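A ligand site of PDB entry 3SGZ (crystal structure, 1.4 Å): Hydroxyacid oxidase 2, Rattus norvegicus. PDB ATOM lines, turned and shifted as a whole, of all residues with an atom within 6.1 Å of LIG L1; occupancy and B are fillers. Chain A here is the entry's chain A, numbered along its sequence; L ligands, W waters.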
ATOM      1  N   PHE A  23      -7.624  17.779  19.188  1.00  0.00           N
ATOM      2  CA  PHE A  23      -8.861  17.401  18.532  1.00  0.00           C
ATOM      3  C   PHE A  23      -8.653  16.107  17.725  1.00  0.00           C
ATOM      4  O   PHE A  23      -9.520  15.202  17.739  1.00  0.00           O
ATOM      5  CB  PHE A  23      -9.349  18.518  17.619  1.00  0.00           C
ATOM      6  CG  PHE A  23     -10.539  18.151  16.809  1.00  0.00           C
ATOM      7  CD1 PHE A  23     -10.440  18.008  15.430  1.00  0.00           C
ATOM      8  CD2 PHE A  23     -11.744  17.866  17.429  1.00  0.00           C
ATOM      9  CE1 PHE A  23     -11.517  17.582  14.666  1.00  0.00           C
ATOM     10  CE2 PHE A  23     -12.838  17.428  16.671  1.00  0.00           C
ATOM     11  CZ  PHE A  23     -12.722  17.284  15.307  1.00  0.00           C
ATOM     12  N   ILE A  24      -7.539  15.995  16.995  1.00  0.00           N
ATOM     13  CA  ILE A  24      -7.291  14.783  16.219  1.00  0.00           C
ATOM     14  C   ILE A  24      -7.096  13.558  17.098  1.00  0.00           C
ATOM     15  O   ILE A  24      -7.534  12.472  16.736  1.00  0.00           O
ATOM     16  CB  ILE A  24      -6.163  15.031  15.192  1.00  0.00           C
ATOM     17  CG1 ILE A  24      -6.672  16.105  14.200  1.00  0.00           C
ATOM     18  CG2 ILE A  24      -5.796  13.719  14.462  1.00  0.00           C
ATOM     19  CD1 ILE A  24      -5.562  16.719  13.263  1.00  0.00           C
ATOM     20  N   GLU A  25      -6.458  13.713  18.258  1.00  0.00           N
ATOM     21  CA  GLU A  25      -6.382  12.593  19.232  1.00  0.00           C
ATOM     22  C   GLU A  25      -7.797  12.388  19.782  1.00  0.00           C
ATOM     23  O   GLU A  25      -8.436  11.342  19.527  1.00  0.00           O
ATOM     24  CB  GLU A  25      -5.436  12.972  20.359  1.00  0.00           C
ATOM     25  CG  GLU A  25      -4.000  12.940  19.848  1.00  0.00           C
ATOM     26  CD  GLU A  25      -3.482  11.525  19.815  1.00  0.00           C
ATOM     27  OE1 GLU A  25      -2.983  11.059  20.867  1.00  0.00           O
ATOM     28  OE2 GLU A  25      -3.614  10.854  18.772  1.00  0.00           O
ATOM     29  N   ASN A  37      -7.517  -0.079  21.361  1.00  0.00           N
ATOM     30  CA  ASN A  37      -7.666  -0.400  19.927  1.00  0.00           C
ATOM     31  C   ASN A  37      -6.341  -0.880  19.361  1.00  0.00           C
ATOM     32  O   ASN A  37      -6.322  -1.713  18.456  1.00  0.00           O
ATOM     33  CB  ASN A  37      -8.158   0.825  19.136  1.00  0.00           C
ATOM     34  CG  ASN A  37      -9.675   1.008  19.228  1.00  0.00           C
ATOM     35  OD1 ASN A  37     -10.392   0.110  19.687  1.00  0.00           O
ATOM     36  ND2 ASN A  37     -10.159   2.161  18.805  1.00  0.00           N
ATOM     37  N   SER A  75     -12.011   6.331   6.532  1.00  0.00           N
ATOM     38  CA  SER A  75     -13.193   6.524   7.374  1.00  0.00           C
ATOM     39  C   SER A  75     -13.554   7.999   7.406  1.00  0.00           C
ATOM     40  O   SER A  75     -12.693   8.879   7.243  1.00  0.00           O
ATOM     41  CB  SER A  75     -12.923   6.056   8.820  1.00  0.00           C
ATOM     42  OG  SER A  75     -13.889   5.035   9.133  1.00  0.00           O
ATOM     43  N   PRO A  76     -14.817   8.312   7.688  1.00  0.00           N
ATOM     44  CA  PRO A  76     -15.250   9.701   7.752  1.00  0.00           C
ATOM     45  C   PRO A  76     -14.620  10.441   8.900  1.00  0.00           C
ATOM     46  O   PRO A  76     -14.725  10.021  10.064  1.00  0.00           O
ATOM     47  CB  PRO A  76     -16.793   9.606   7.895  1.00  0.00           C
ATOM     48  CG  PRO A  76     -17.000   8.248   8.529  1.00  0.00           C
ATOM     49  CD  PRO A  76     -15.918   7.355   7.904  1.00  0.00           C
ATOM     50  N   THR A  77     -13.942  11.557   8.599  1.00  0.00           N
ATOM     51  CA  THR A  77     -13.330  12.377   9.643  1.00  0.00           C
ATOM     52  C   THR A  77     -13.620  13.817   9.295  1.00  0.00           C
ATOM     53  O   THR A  77     -13.393  14.249   8.158  1.00  0.00           O
ATOM     54  CB  THR A  77     -11.793  12.158   9.734  1.00  0.00           C
ATOM     55  OG1 THR A  77     -11.245  12.121   8.425  1.00  0.00           O
ATOM     56  CG2 THR A  77     -11.464  10.846  10.418  1.00  0.00           C
ATOM     57  N   ALA A  78     -14.166  14.559  10.256  1.00  0.00           N
ATOM     58  CA  ALA A  78     -14.513  15.973  10.048  1.00  0.00           C
ATOM     59  C   ALA A  78     -13.349  16.922   9.834  1.00  0.00           C
ATOM     60  O   ALA A  78     -12.223  16.663  10.256  1.00  0.00           O
ATOM     61  CB  ALA A  78     -15.291  16.451  11.250  1.00  0.00           C
ATOM     62  N   SER A 105     -16.979  12.966   5.370  1.00  0.00           N
ATOM     63  CA  SER A 105     -17.707  13.296   6.600  1.00  0.00           C
ATOM     64  C   SER A 105     -18.835  14.262   6.360  1.00  0.00           C
ATOM     65  O   SER A 105     -18.823  15.046   5.426  1.00  0.00           O
ATOM     66  CB  SER A 105     -16.766  13.930   7.617  1.00  0.00           C
ATOM     67  OG  SER A 105     -17.451  14.568   8.705  1.00  0.00           O
ATOM     68  N   SER A 106     -19.762  14.231   7.307  1.00  0.00           N
ATOM     69  CA  SER A 106     -20.919  15.094   7.319  1.00  0.00           C
ATOM     70  C   SER A 106     -20.513  16.535   7.678  1.00  0.00           C
ATOM     71  O   SER A 106     -21.293  17.482   7.523  1.00  0.00           O
ATOM     72  CB  SER A 106     -21.915  14.555   8.339  1.00  0.00           C
ATOM     73  OG  SER A 106     -23.111  15.277   8.312  1.00  0.00           O
ATOM     74  N   TYR A 107     -19.288  16.683   8.154  1.00  0.00           N
ATOM     75  CA  TYR A 107     -18.758  17.984   8.558  1.00  0.00           C
ATOM     76  C   TYR A 107     -17.453  18.274   7.864  1.00  0.00           C
ATOM     77  O   TYR A 107     -16.430  18.547   8.496  1.00  0.00           O
ATOM     78  CB  TYR A 107     -18.545  18.022  10.053  1.00  0.00           C
ATOM     79  CG  TYR A 107     -19.839  18.077  10.803  1.00  0.00           C
ATOM     80  CD1 TYR A 107     -20.573  19.265  10.852  1.00  0.00           C
ATOM     81  CD2 TYR A 107     -20.312  16.970  11.480  1.00  0.00           C
ATOM     82  CE1 TYR A 107     -21.756  19.341  11.557  1.00  0.00           C
ATOM     83  CE2 TYR A 107     -21.507  17.029  12.199  1.00  0.00           C
ATOM     84  CZ  TYR A 107     -22.217  18.225  12.234  1.00  0.00           C
ATOM     85  OH  TYR A 107     -23.372  18.329  12.991  1.00  0.00           O
ATOM     86  N   GLN A 127     -21.013  10.128   4.639  1.00  0.00           N
ATOM     87  CA  GLN A 127     -21.524   9.891   5.981  1.00  0.00           C
ATOM     88  C   GLN A 127     -22.345  11.114   6.338  1.00  0.00           C
ATOM     89  O   GLN A 127     -21.831  12.221   6.391  1.00  0.00           O
ATOM     90  CB  GLN A 127     -20.344   9.716   6.951  1.00  0.00           C
ATOM     91  CG  GLN A 127     -20.761   9.419   8.409  1.00  0.00           C
ATOM     92  CD  GLN A 127     -20.815  10.674   9.271  1.00  0.00           C
ATOM     93  OE1 GLN A 127     -19.879  11.482   9.258  1.00  0.00           O
ATOM     94  NE2 GLN A 127     -21.895  10.859  10.032  1.00  0.00           N
ATOM     95  N   TYR A 129     -24.988  12.943   9.083  1.00  0.00           N
ATOM     96  CA  TYR A 129     -25.667  12.978  10.352  1.00  0.00           C
ATOM     97  C   TYR A 129     -27.042  13.571  10.012  1.00  0.00           C
ATOM     98  O   TYR A 129     -27.135  14.672   9.454  1.00  0.00           O
ATOM     99  CB  TYR A 129     -24.938  13.875  11.352  1.00  0.00           C
ATOM    100  CG  TYR A 129     -23.796  13.187  12.036  1.00  0.00           C
ATOM    101  CD1 TYR A 129     -22.487  13.647  11.883  1.00  0.00           C
ATOM    102  CD2 TYR A 129     -24.003  12.055  12.857  1.00  0.00           C
ATOM    103  CE1 TYR A 129     -21.412  13.022  12.515  1.00  0.00           C
ATOM    104  CE2 TYR A 129     -22.933  11.409  13.483  1.00  0.00           C
ATOM    105  CZ  TYR A 129     -21.641  11.907  13.308  1.00  0.00           C
ATOM    106  OH  TYR A 129     -20.552  11.298  13.899  1.00  0.00           O
ATOM    107  N   VAL A 153     -23.258   6.343   4.670  1.00  0.00           N
ATOM    108  CA  VAL A 153     -22.825   5.779   5.937  1.00  0.00           C
ATOM    109  C   VAL A 153     -23.568   6.544   7.032  1.00  0.00           C
ATOM    110  O   VAL A 153     -23.573   7.789   7.075  1.00  0.00           O
ATOM    111  CB  VAL A 153     -21.299   5.947   6.098  1.00  0.00           C
ATOM    112  CG1 VAL A 153     -20.860   5.532   7.517  1.00  0.00           C
ATOM    113  CG2 VAL A 153     -20.606   5.104   5.078  1.00  0.00           C
ATOM    114  N   THR A 155     -23.598   6.965  10.973  1.00  0.00           N
ATOM    115  CA  THR A 155     -22.798   6.694  12.189  1.00  0.00           C
ATOM    116  C   THR A 155     -23.784   6.733  13.333  1.00  0.00           C
ATOM    117  O   THR A 155     -24.506   7.710  13.499  1.00  0.00           O
ATOM    118  CB  THR A 155     -21.750   7.760  12.326  1.00  0.00           C
ATOM    119  OG1 THR A 155     -20.842   7.602  11.241  1.00  0.00           O
ATOM    120  CG2 THR A 155     -20.988   7.585  13.655  1.00  0.00           C
ATOM    121  N   ASP A 157     -23.056   5.897  16.765  1.00  0.00           N
ATOM    122  CA  ASP A 157     -22.502   5.956  18.112  1.00  0.00           C
ATOM    123  C   ASP A 157     -22.265   7.337  18.647  1.00  0.00           C
ATOM    124  O   ASP A 157     -21.581   7.504  19.654  1.00  0.00           O
ATOM    125  CB  ASP A 157     -21.215   5.094  18.168  1.00  0.00           C
ATOM    126  CG  ASP A 157     -20.129   5.566  17.207  1.00  0.00           C
ATOM    127  OD1 ASP A 157     -19.139   4.792  17.027  1.00  0.00           O
ATOM    128  OD2 ASP A 157     -20.245   6.695  16.656  1.00  0.00           O
ATOM    129  N   THR A 158     -22.869   8.328  17.997  1.00  0.00           N
ATOM    130  CA  THR A 158     -22.707   9.721  18.360  1.00  0.00           C
ATOM    131  C   THR A 158     -24.033  10.489  18.555  1.00  0.00           C
ATOM    132  O   THR A 158     -24.262  11.518  17.934  1.00  0.00           O
ATOM    133  CB  THR A 158     -21.794  10.408  17.296  1.00  0.00           C
ATOM    134  OG1 THR A 158     -20.665   9.548  17.085  1.00  0.00           O
ATOM    135  CG2 THR A 158     -21.301  11.794  17.764  1.00  0.00           C
ATOM    136  N   LYS A 223     -22.349   2.534  10.832  1.00  0.00           N
ATOM    137  CA  LYS A 223     -21.008   2.606  11.424  1.00  0.00           C
ATOM    138  C   LYS A 223     -21.118   2.788  12.930  1.00  0.00           C
ATOM    139  O   LYS A 223     -21.825   3.678  13.420  1.00  0.00           O
ATOM    140  CB  LYS A 223     -20.254   3.793  10.787  1.00  0.00           C
ATOM    141  CG  LYS A 223     -18.931   4.133  11.454  1.00  0.00           C
ATOM    142  CD  LYS A 223     -18.150   5.141  10.553  1.00  0.00           C
ATOM    143  CE  LYS A 223     -16.804   5.538  11.221  1.00  0.00           C
ATOM    144  NZ  LYS A 223     -16.986   6.528  12.328  1.00  0.00           N
ATOM    145  N   SER A 245     -16.926  -0.421  14.836  1.00  0.00           N
ATOM    146  CA  SER A 245     -16.141   0.736  15.198  1.00  0.00           C
ATOM    147  C   SER A 245     -16.567   1.212  16.563  1.00  0.00           C
ATOM    148  O   SER A 245     -17.737   1.086  16.933  1.00  0.00           O
ATOM    149  CB  SER A 245     -16.470   1.854  14.193  1.00  0.00           C
ATOM    150  OG  SER A 245     -15.844   3.127  14.508  1.00  0.00           O
ATOM    151  N   ASN A 246     -15.628   1.773  17.331  1.00  0.00           N
ATOM    152  CA  ASN A 246     -15.939   2.431  18.590  1.00  0.00           C
ATOM    153  C   ASN A 246     -15.594   3.926  18.432  1.00  0.00           C
ATOM    154  O   ASN A 246     -15.332   4.643  19.403  1.00  0.00           O
ATOM    155  CB  ASN A 246     -15.209   1.805  19.790  1.00  0.00           C
ATOM    156  CG  ASN A 246     -13.757   1.638  19.561  1.00  0.00           C
ATOM    157  OD1 ASN A 246     -13.110   2.506  18.957  1.00  0.00           O
ATOM    158  ND2 ASN A 246     -13.209   0.512  19.995  1.00  0.00           N
ATOM    159  N   HIS A 247     -15.565   4.405  17.181  1.00  0.00           N
ATOM    160  CA  HIS A 247     -15.286   5.829  16.920  1.00  0.00           C
ATOM    161  C   HIS A 247     -13.905   6.220  17.447  1.00  0.00           C
ATOM    162  O   HIS A 247     -13.696   7.342  17.907  1.00  0.00           O
ATOM    163  CB  HIS A 247     -16.419   6.686  17.534  1.00  0.00           C
ATOM    164  CG  HIS A 247     -16.717   7.979  16.802  1.00  0.00           C
ATOM    165  ND1 HIS A 247     -17.909   8.161  16.135  1.00  0.00           N
ATOM    166  CD2 HIS A 247     -16.030   9.153  16.693  1.00  0.00           C
ATOM    167  CE1 HIS A 247     -17.946   9.403  15.646  1.00  0.00           C
ATOM    168  NE2 HIS A 247     -16.822  10.011  15.969  1.00  0.00           N
ATOM    169  N   GLY A 248     -12.966   5.293  17.369  1.00  0.00           N
ATOM    170  CA  GLY A 248     -11.612   5.597  17.795  1.00  0.00           C
ATOM    171  C   GLY A 248     -11.459   5.901  19.257  1.00  0.00           C
ATOM    172  O   GLY A 248     -10.516   6.587  19.653  1.00  0.00           O
ATOM    173  N   GLY A 249     -12.356   5.397  20.098  1.00  0.00           N
ATOM    174  CA  GLY A 249     -12.276   5.707  21.522  1.00  0.00           C
ATOM    175  C   GLY A 249     -12.574   7.173  21.833  1.00  0.00           C
ATOM    176  O   GLY A 249     -12.179   7.666  22.905  1.00  0.00           O
ATOM    177  N   ARG A 250     -13.303   7.858  20.946  1.00  0.00           N
ATOM    178  CA  ARG A 250     -13.647   9.266  21.106  1.00  0.00           C
ATOM    179  C   ARG A 250     -15.088   9.473  21.640  1.00  0.00           C
ATOM    180  O   ARG A 250     -15.467  10.618  21.921  1.00  0.00           O
ATOM    181  CB  ARG A 250     -13.578   9.968  19.733  1.00  0.00           C
ATOM    182  CG  ARG A 250     -12.185   9.921  19.122  1.00  0.00           C
ATOM    183  CD  ARG A 250     -12.218  10.355  17.670  1.00  0.00           C
ATOM    184  NE  ARG A 250     -12.603  11.738  17.403  1.00  0.00           N
ATOM    185  CZ  ARG A 250     -11.743  12.757  17.447  1.00  0.00           C
ATOM    186  NH1 ARG A 250     -10.487  12.532  17.804  1.00  0.00           N
ATOM    187  NH2 ARG A 250     -12.098  13.956  16.980  1.00  0.00           N
ATOM    188  N   ASP A 278     -12.987  -0.180  11.661  1.00  0.00           N
ATOM    189  CA  ASP A 278     -11.929   0.828  11.826  1.00  0.00           C
ATOM    190  C   ASP A 278     -11.536   0.824  13.299  1.00  0.00           C
ATOM    191  O   ASP A 278     -12.186   0.180  14.147  1.00  0.00           O
ATOM    192  CB  ASP A 278     -12.322   2.240  11.318  1.00  0.00           C
ATOM    193  CG  ASP A 278     -13.339   2.953  12.176  1.00  0.00           C
ATOM    194  OD1 ASP A 278     -13.902   3.933  11.654  1.00  0.00           O
ATOM    195  OD2 ASP A 278     -13.561   2.603  13.357  1.00  0.00           O
ATOM    196  N   GLY A 279     -10.434   1.511  13.602  1.00  0.00           N
ATOM    197  CA  GLY A 279      -9.984   1.668  14.960  1.00  0.00           C
ATOM    198  C   GLY A 279      -8.659   1.039  15.263  1.00  0.00           C
ATOM    199  O   GLY A 279      -8.571  -0.178  15.479  1.00  0.00           O
ATOM    200  N   GLY A 280      -7.595   1.842  15.219  1.00  0.00           N
ATOM    201  CA  GLY A 280      -6.278   1.313  15.587  1.00  0.00           C
ATOM    202  C   GLY A 280      -5.495   0.630  14.509  1.00  0.00           C
ATOM    203  O   GLY A 280      -4.464   0.051  14.815  1.00  0.00           O
ATOM    204  N   VAL A 281      -5.942   0.687  13.247  1.00  0.00           N
ATOM    205  CA  VAL A 281      -5.193   0.053  12.154  1.00  0.00           C
ATOM    206  C   VAL A 281      -3.995   0.958  11.806  1.00  0.00           C
ATOM    207  O   VAL A 281      -4.196   2.106  11.372  1.00  0.00           O
ATOM    208  CB  VAL A 281      -6.058  -0.133  10.914  1.00  0.00           C
ATOM    209  CG1 VAL A 281      -5.227  -0.726   9.782  1.00  0.00           C
ATOM    210  CG2 VAL A 281      -7.267  -1.054  11.233  1.00  0.00           C
ATOM    211  N   ARG A 282      -2.787   0.442  12.014  1.00  0.00           N
ATOM    212  CA  ARG A 282      -1.582   1.251  11.785  1.00  0.00           C
ATOM    213  C   ARG A 282      -0.516   0.524  10.993  1.00  0.00           C
ATOM    214  O   ARG A 282       0.365   1.186  10.423  1.00  0.00           O
ATOM    215  CB  ARG A 282      -0.956   1.665  13.119  1.00  0.00           C
ATOM    216  CG  ARG A 282      -1.924   2.389  14.056  1.00  0.00           C
ATOM    217  CD  ARG A 282      -2.380   3.748  13.538  1.00  0.00           C
ATOM    218  NE  ARG A 282      -3.319   4.391  14.461  1.00  0.00           N
ATOM    219  CZ  ARG A 282      -4.639   4.545  14.249  1.00  0.00           C
ATOM    220  NH1 ARG A 282      -5.229   4.070  13.142  1.00  0.00           N
ATOM    221  NH2 ARG A 282      -5.327   5.244  15.126  1.00  0.00           N
ATOM    222  N   PHE A 299     -10.998   0.642   7.478  1.00  0.00           N
ATOM    223  CA  PHE A 299     -11.019   2.084   7.205  1.00  0.00           C
ATOM    224  C   PHE A 299     -10.071   2.739   8.188  1.00  0.00           C
ATOM    225  O   PHE A 299      -9.887   2.285   9.334  1.00  0.00           O
ATOM    226  CB  PHE A 299     -12.427   2.664   7.394  1.00  0.00           C
ATOM    227  CG  PHE A 299     -13.399   2.227   6.322  1.00  0.00           C
ATOM    228  CD1 PHE A 299     -13.963   0.956   6.348  1.00  0.00           C
ATOM    229  CD2 PHE A 299     -13.704   3.072   5.263  1.00  0.00           C
ATOM    230  CE1 PHE A 299     -14.833   0.518   5.323  1.00  0.00           C
ATOM    231  CE2 PHE A 299     -14.569   2.654   4.259  1.00  0.00           C
ATOM    232  CZ  PHE A 299     -15.133   1.371   4.279  1.00  0.00           C
ATOM    233  N   LEU A 300      -9.444   3.801   7.700  1.00  0.00           N
ATOM    234  CA  LEU A 300      -8.493   4.599   8.473  1.00  0.00           C
ATOM    235  C   LEU A 300      -9.077   5.935   8.855  1.00  0.00           C
ATOM    236  O   LEU A 300      -9.628   6.651   8.004  1.00  0.00           O
ATOM    237  CB  LEU A 300      -7.239   4.884   7.635  1.00  0.00           C
ATOM    238  CG  LEU A 300      -6.438   3.679   7.207  1.00  0.00           C
ATOM    239  CD1 LEU A 300      -5.319   4.137   6.282  1.00  0.00           C
ATOM    240  CD2 LEU A 300      -5.808   3.000   8.423  1.00  0.00           C
ATOM    241  N   GLY A 301      -8.915   6.316  10.107  1.00  0.00           N
ATOM    242  CA  GLY A 301      -9.377   7.597  10.599  1.00  0.00           C
ATOM    243  C   GLY A 301      -8.202   8.560  10.718  1.00  0.00           C
ATOM    244  O   GLY A 301      -7.825   9.244   9.740  1.00  0.00           O
ATOM    245  N   ARG A 302      -7.589   8.597  11.897  1.00  0.00           N
ATOM    246  CA  ARG A 302      -6.472   9.509  12.140  1.00  0.00           C
ATOM    247  C   ARG A 302      -5.279   9.462  11.167  1.00  0.00           C
ATOM    248  O   ARG A 302      -4.773  10.519  10.809  1.00  0.00           O
ATOM    249  CB  ARG A 302      -5.946   9.325  13.573  1.00  0.00           C
ATOM    250  CG  ARG A 302      -6.966   9.676  14.622  1.00  0.00           C
ATOM    251  CD  ARG A 302      -6.450   9.343  16.002  1.00  0.00           C
ATOM    252  NE  ARG A 302      -7.445   9.525  17.099  1.00  0.00           N
ATOM    253  CZ  ARG A 302      -8.266   8.555  17.524  1.00  0.00           C
ATOM    254  NH1 ARG A 302      -8.250   7.365  16.924  1.00  0.00           N
ATOM    255  NH2 ARG A 302      -8.960   8.744  18.633  1.00  0.00           N
ATOM    256  N   PRO A 303      -4.879   8.288  10.660  1.00  0.00           N
ATOM    257  CA  PRO A 303      -3.712   8.293   9.764  1.00  0.00           C
ATOM    258  C   PRO A 303      -3.872   9.165   8.541  1.00  0.00           C
ATOM    259  O   PRO A 303      -2.872   9.703   8.017  1.00  0.00           O
ATOM    260  CB  PRO A 303      -3.506   6.820   9.421  1.00  0.00           C
ATOM    261  CG  PRO A 303      -4.017   6.119  10.698  1.00  0.00           C
ATOM    262  CD  PRO A 303      -5.277   6.908  11.009  1.00  0.00           C
ATOM    263  N   LEU A 305      -5.502  12.059   8.429  1.00  0.00           N
ATOM    264  CA  LEU A 305      -5.269  13.409   8.907  1.00  0.00           C
ATOM    265  C   LEU A 305      -3.764  13.600   9.153  1.00  0.00           C
ATOM    266  O   LEU A 305      -3.238  14.700   8.889  1.00  0.00           O
ATOM    267  CB  LEU A 305      -6.075  13.669  10.196  1.00  0.00           C
ATOM    268  CG  LEU A 305      -7.588  13.383   9.984  1.00  0.00           C
ATOM    269  CD1 LEU A 305      -8.348  13.573  11.281  1.00  0.00           C
ATOM    270  CD2 LEU A 305      -8.176  14.295   8.915  1.00  0.00           C
HETATM  271  N1  LIG L   1     -16.599   9.539  12.544  1.00  0.00           N
HETATM  272  C1  LIG L   1     -17.755   9.770  11.852  1.00  0.00           C
HETATM  273  O1  LIG L   1     -18.526   8.881  11.608  1.00  0.00           O
HETATM  274  N2  LIG L   1     -17.927  11.118  11.444  1.00  0.00           N
HETATM  275  C2  LIG L   1     -17.068  12.179  11.666  1.00  0.00           C
HETATM  276  O2  LIG L   1     -17.390  13.279  11.212  1.00  0.00           O
HETATM  277  C3  LIG L   1     -15.914  11.813  12.377  1.00  0.00           C
HETATM  278  N3  LIG L   1     -15.002  12.849  12.572  1.00  0.00           N
HETATM  279  C4  LIG L   1     -13.785  12.505  13.166  1.00  0.00           C
HETATM  280  C5  LIG L   1     -12.830  13.514  13.298  1.00  0.00           C
HETATM  281  C6  LIG L   1     -11.562  13.188  13.781  1.00  0.00           C
HETATM  282  C7  LIG L   1     -10.524  14.299  13.869  1.00  0.00           C
HETATM  283  C8  LIG L   1     -11.262  11.861  14.159  1.00  0.00           C
HETATM  284  C9  LIG L   1      -9.897  11.465  14.638  1.00  0.00           C
HETATM  285  C10 LIG L   1     -12.213  10.847  14.076  1.00  0.00           C
HETATM  286  C11 LIG L   1     -13.497  11.149  13.578  1.00  0.00           C
HETATM  287  N4  LIG L   1     -14.491  10.145  13.409  1.00  0.00           N
HETATM  288  C12 LIG L   1     -15.673  10.477  12.795  1.00  0.00           C
HETATM  289  C13 LIG L   1     -14.277   8.782  13.776  1.00  0.00           C
HETATM  290  C14 LIG L   1     -13.447   8.029  12.649  1.00  0.00           C
HETATM  291  O3  LIG L   1     -14.335   7.755  11.540  1.00  0.00           O
HETATM  292  C15 LIG L   1     -12.859   6.704  13.059  1.00  0.00           C
HETATM  293  O4  LIG L   1     -13.999   5.872  13.573  1.00  0.00           O
HETATM  294  C16 LIG L   1     -11.913   6.752  14.159  1.00  0.00           C
HETATM  295  O5  LIG L   1     -10.935   7.820  13.989  1.00  0.00           O
HETATM  296  C17 LIG L   1     -11.188   5.420  14.461  1.00  0.00           C
HETATM  297  O6  LIG L   1     -10.173   5.110  13.413  1.00  0.00           O
HETATM  298  P1  LIG L   1      -8.616   5.423  13.691  1.00  0.00           P
HETATM  299  O7  LIG L   1      -8.170   4.583  14.855  1.00  0.00           O
HETATM  300  O8  LIG L   1      -8.433   6.891  13.986  1.00  0.00           O
HETATM  301  O9  LIG L   1      -8.003   4.980  12.427  1.00  0.00           O
HETATM  302  C1  LG2 L   2     -19.928  19.539  15.248  1.00  0.00           C
HETATM  303  N1  LG2 L   2     -17.631  12.759  15.079  1.00  0.00           N
HETATM  304  O1  LG2 L   2     -15.251  12.303  16.346  1.00  0.00           O
HETATM  305  S1  LG2 L   2     -16.468  16.551  15.679  1.00  0.00           S
HETATM  306  C2  LG2 L   2     -19.536  19.151  16.538  1.00  0.00           C
HETATM  307  N2  LG2 L   2     -18.804  13.252  14.568  1.00  0.00           N
HETATM  308  O2  LG2 L   2     -14.727  14.415  16.304  1.00  0.00           O
HETATM  309  S2  LG2 L   2     -18.826  14.931  14.532  1.00  0.00           S
HETATM  310  C3  LG2 L   2     -18.467  18.232  16.684  1.00  0.00           C
HETATM  311  C4  LG2 L   2     -17.819  17.709  15.540  1.00  0.00           C
HETATM  312  C5  LG2 L   2     -18.229  18.122  14.264  1.00  0.00           C
HETATM  313  C6  LG2 L   2     -19.286  19.045  14.111  1.00  0.00           C
HETATM  314  C7  LG2 L   2     -17.191  15.008  15.001  1.00  0.00           C
HETATM  315  C8  LG2 L   2     -16.729  13.834  15.402  1.00  0.00           C
HETATM  316  C9  LG2 L   2     -15.486  13.493  16.061  1.00  0.00           C
HETATM  317  C10 LG2 L   2     -21.205  20.637  14.991  1.00  0.00           C
HETATM  318  O   HOH W   1      -8.582   4.375  17.553  1.00  0.00           O
HETATM  319  O   HOH W   2      -8.393   2.336  11.778  1.00  0.00           O
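The guanidinium group (NH2) of Arg 282 lies within salt-bridge range of an oxygen (O7) of LIG L1 (2.9 Å).
The backbone NH of Gly 280 is in hydrogen-bond range of an oxygen (O7) of LIG L1, 2.8 Å away.
An oxygen (O8) of LIG L1 is in hydrogen-bond range of the backbone NH of Arg 302, at 2.8 Å.
The side-chain carboxylate (OD1) of Asp 278 sits at hydrogen-bond distance from an oxygen (O4) of LIG L1, 2.7 Å away.
The side-chain hydroxyl of Tyr 129 sits at hydrogen-bond distance from a nitrogen (N2) of LG2 L2, at 2.7 Å.
O of Pro 76 lies within hydrogen-bond range of O3 of LIG L1, at 2.7 Å.
The guanidinium group (NH1) of Arg 302 lies within salt-bridge range of an oxygen (O8) of LIG L1.
A ring nitrogen (NE2) of His 247 sits close to a nitrogen (N1) of LIG L1 (3.5 Å).
The backbone NH of Gly 301 sits at hydrogen-bond distance from an oxygen (O9) of LIG L1 (2.8 Å).
A nitrogen (N3) of LIG L1 sits at hydrogen-bond distance from the backbone NH (N) of Ala 78.
The side-chain amino group (NZ) of Lys 223 sits at hydrogen-bond distance from an oxygen (O1) of LIG L1.
The guanidinium group of Arg 250 lies within salt-bridge range of an oxygen (O2) of LG2 L2.
The side-chain amide oxygen of Gln 127 sits at hydrogen-bond distance from a nitrogen (N2) of LIG L1 (3.0 Å).
OG1 of Thr 155 lies within hydrogen-bond range of O1 of LIG L1.
O4 of LIG L1 sits at hydrogen-bond distance from OG of Ser 245 (3.4 Å).
The side-chain hydroxyl (OG) of Ser 105 is in hydrogen-bond range of an oxygen (O2) of LIG L1.
NE2 of His 247 is in hydrogen-bond range of O1 of LG2 L2, 2.8 Å away.
The backbone carbonyl oxygen (O) of Gly 248 lies within hydrogen-bond range of the guanidinium group (NH2) of Arg 302.
OG of Ser 245 is in hydrogen-bond range of OD2 of Asp 278 (2.6 Å).
ND1 of His 247 lies close to OG1 of Thr 158 (3.2 Å).
The backbone carbonyl oxygen of Gln 127 lies within hydrogen-bond range of the backbone NH of Ser 106 (3.0 Å).
The backbone NH (N) of His 247 lies within hydrogen-bond range of the side-chain hydroxyl (OG) of Ser 245 (3.0 Å).
O of Glu 25 is in hydrogen-bond range of NH1 of Arg 250, at 2.9 Å.
The side-chain carboxylate (OD2) of Asp 157 lies within hydrogen-bond range of a ring nitrogen (ND1) of His 247 (2.8 Å).
NH1 of Arg 250 sits at hydrogen-bond distance from O of Ile 24, at 3.1 Å.
Residues that only touch LIG L1: Ile 24 (3.3 Å), Arg 250 (3.3 Å), Gly 248 (3.4 Å), Thr 77 (3.4 Å), Gly 279 (3.4 Å), Leu 305 (3.5 Å), Ser 75 (3.5 Å), Phe 23 (3.5 Å), Tyr 129 (3.6 Å), Pro 303 (3.6 Å) and Leu 300 (3.9 Å).
Hydrophobic or aromatic side chains that line LIG L1: Phe 23, Pro 76, Ala 78, His 247, Pro 303 and Leu 305.
Water W1 lies within hydrogen-bond range of O7 of LIG L1 (2.7 Å), ND2 of Asn 37 (3.0 Å) and NH1 of Arg 302 (3.1 Å).
Water W2 lies within hydrogen-bond range of O9 of LIG L1, N of Gly 279, O of Phe 299 and N of Val 281.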
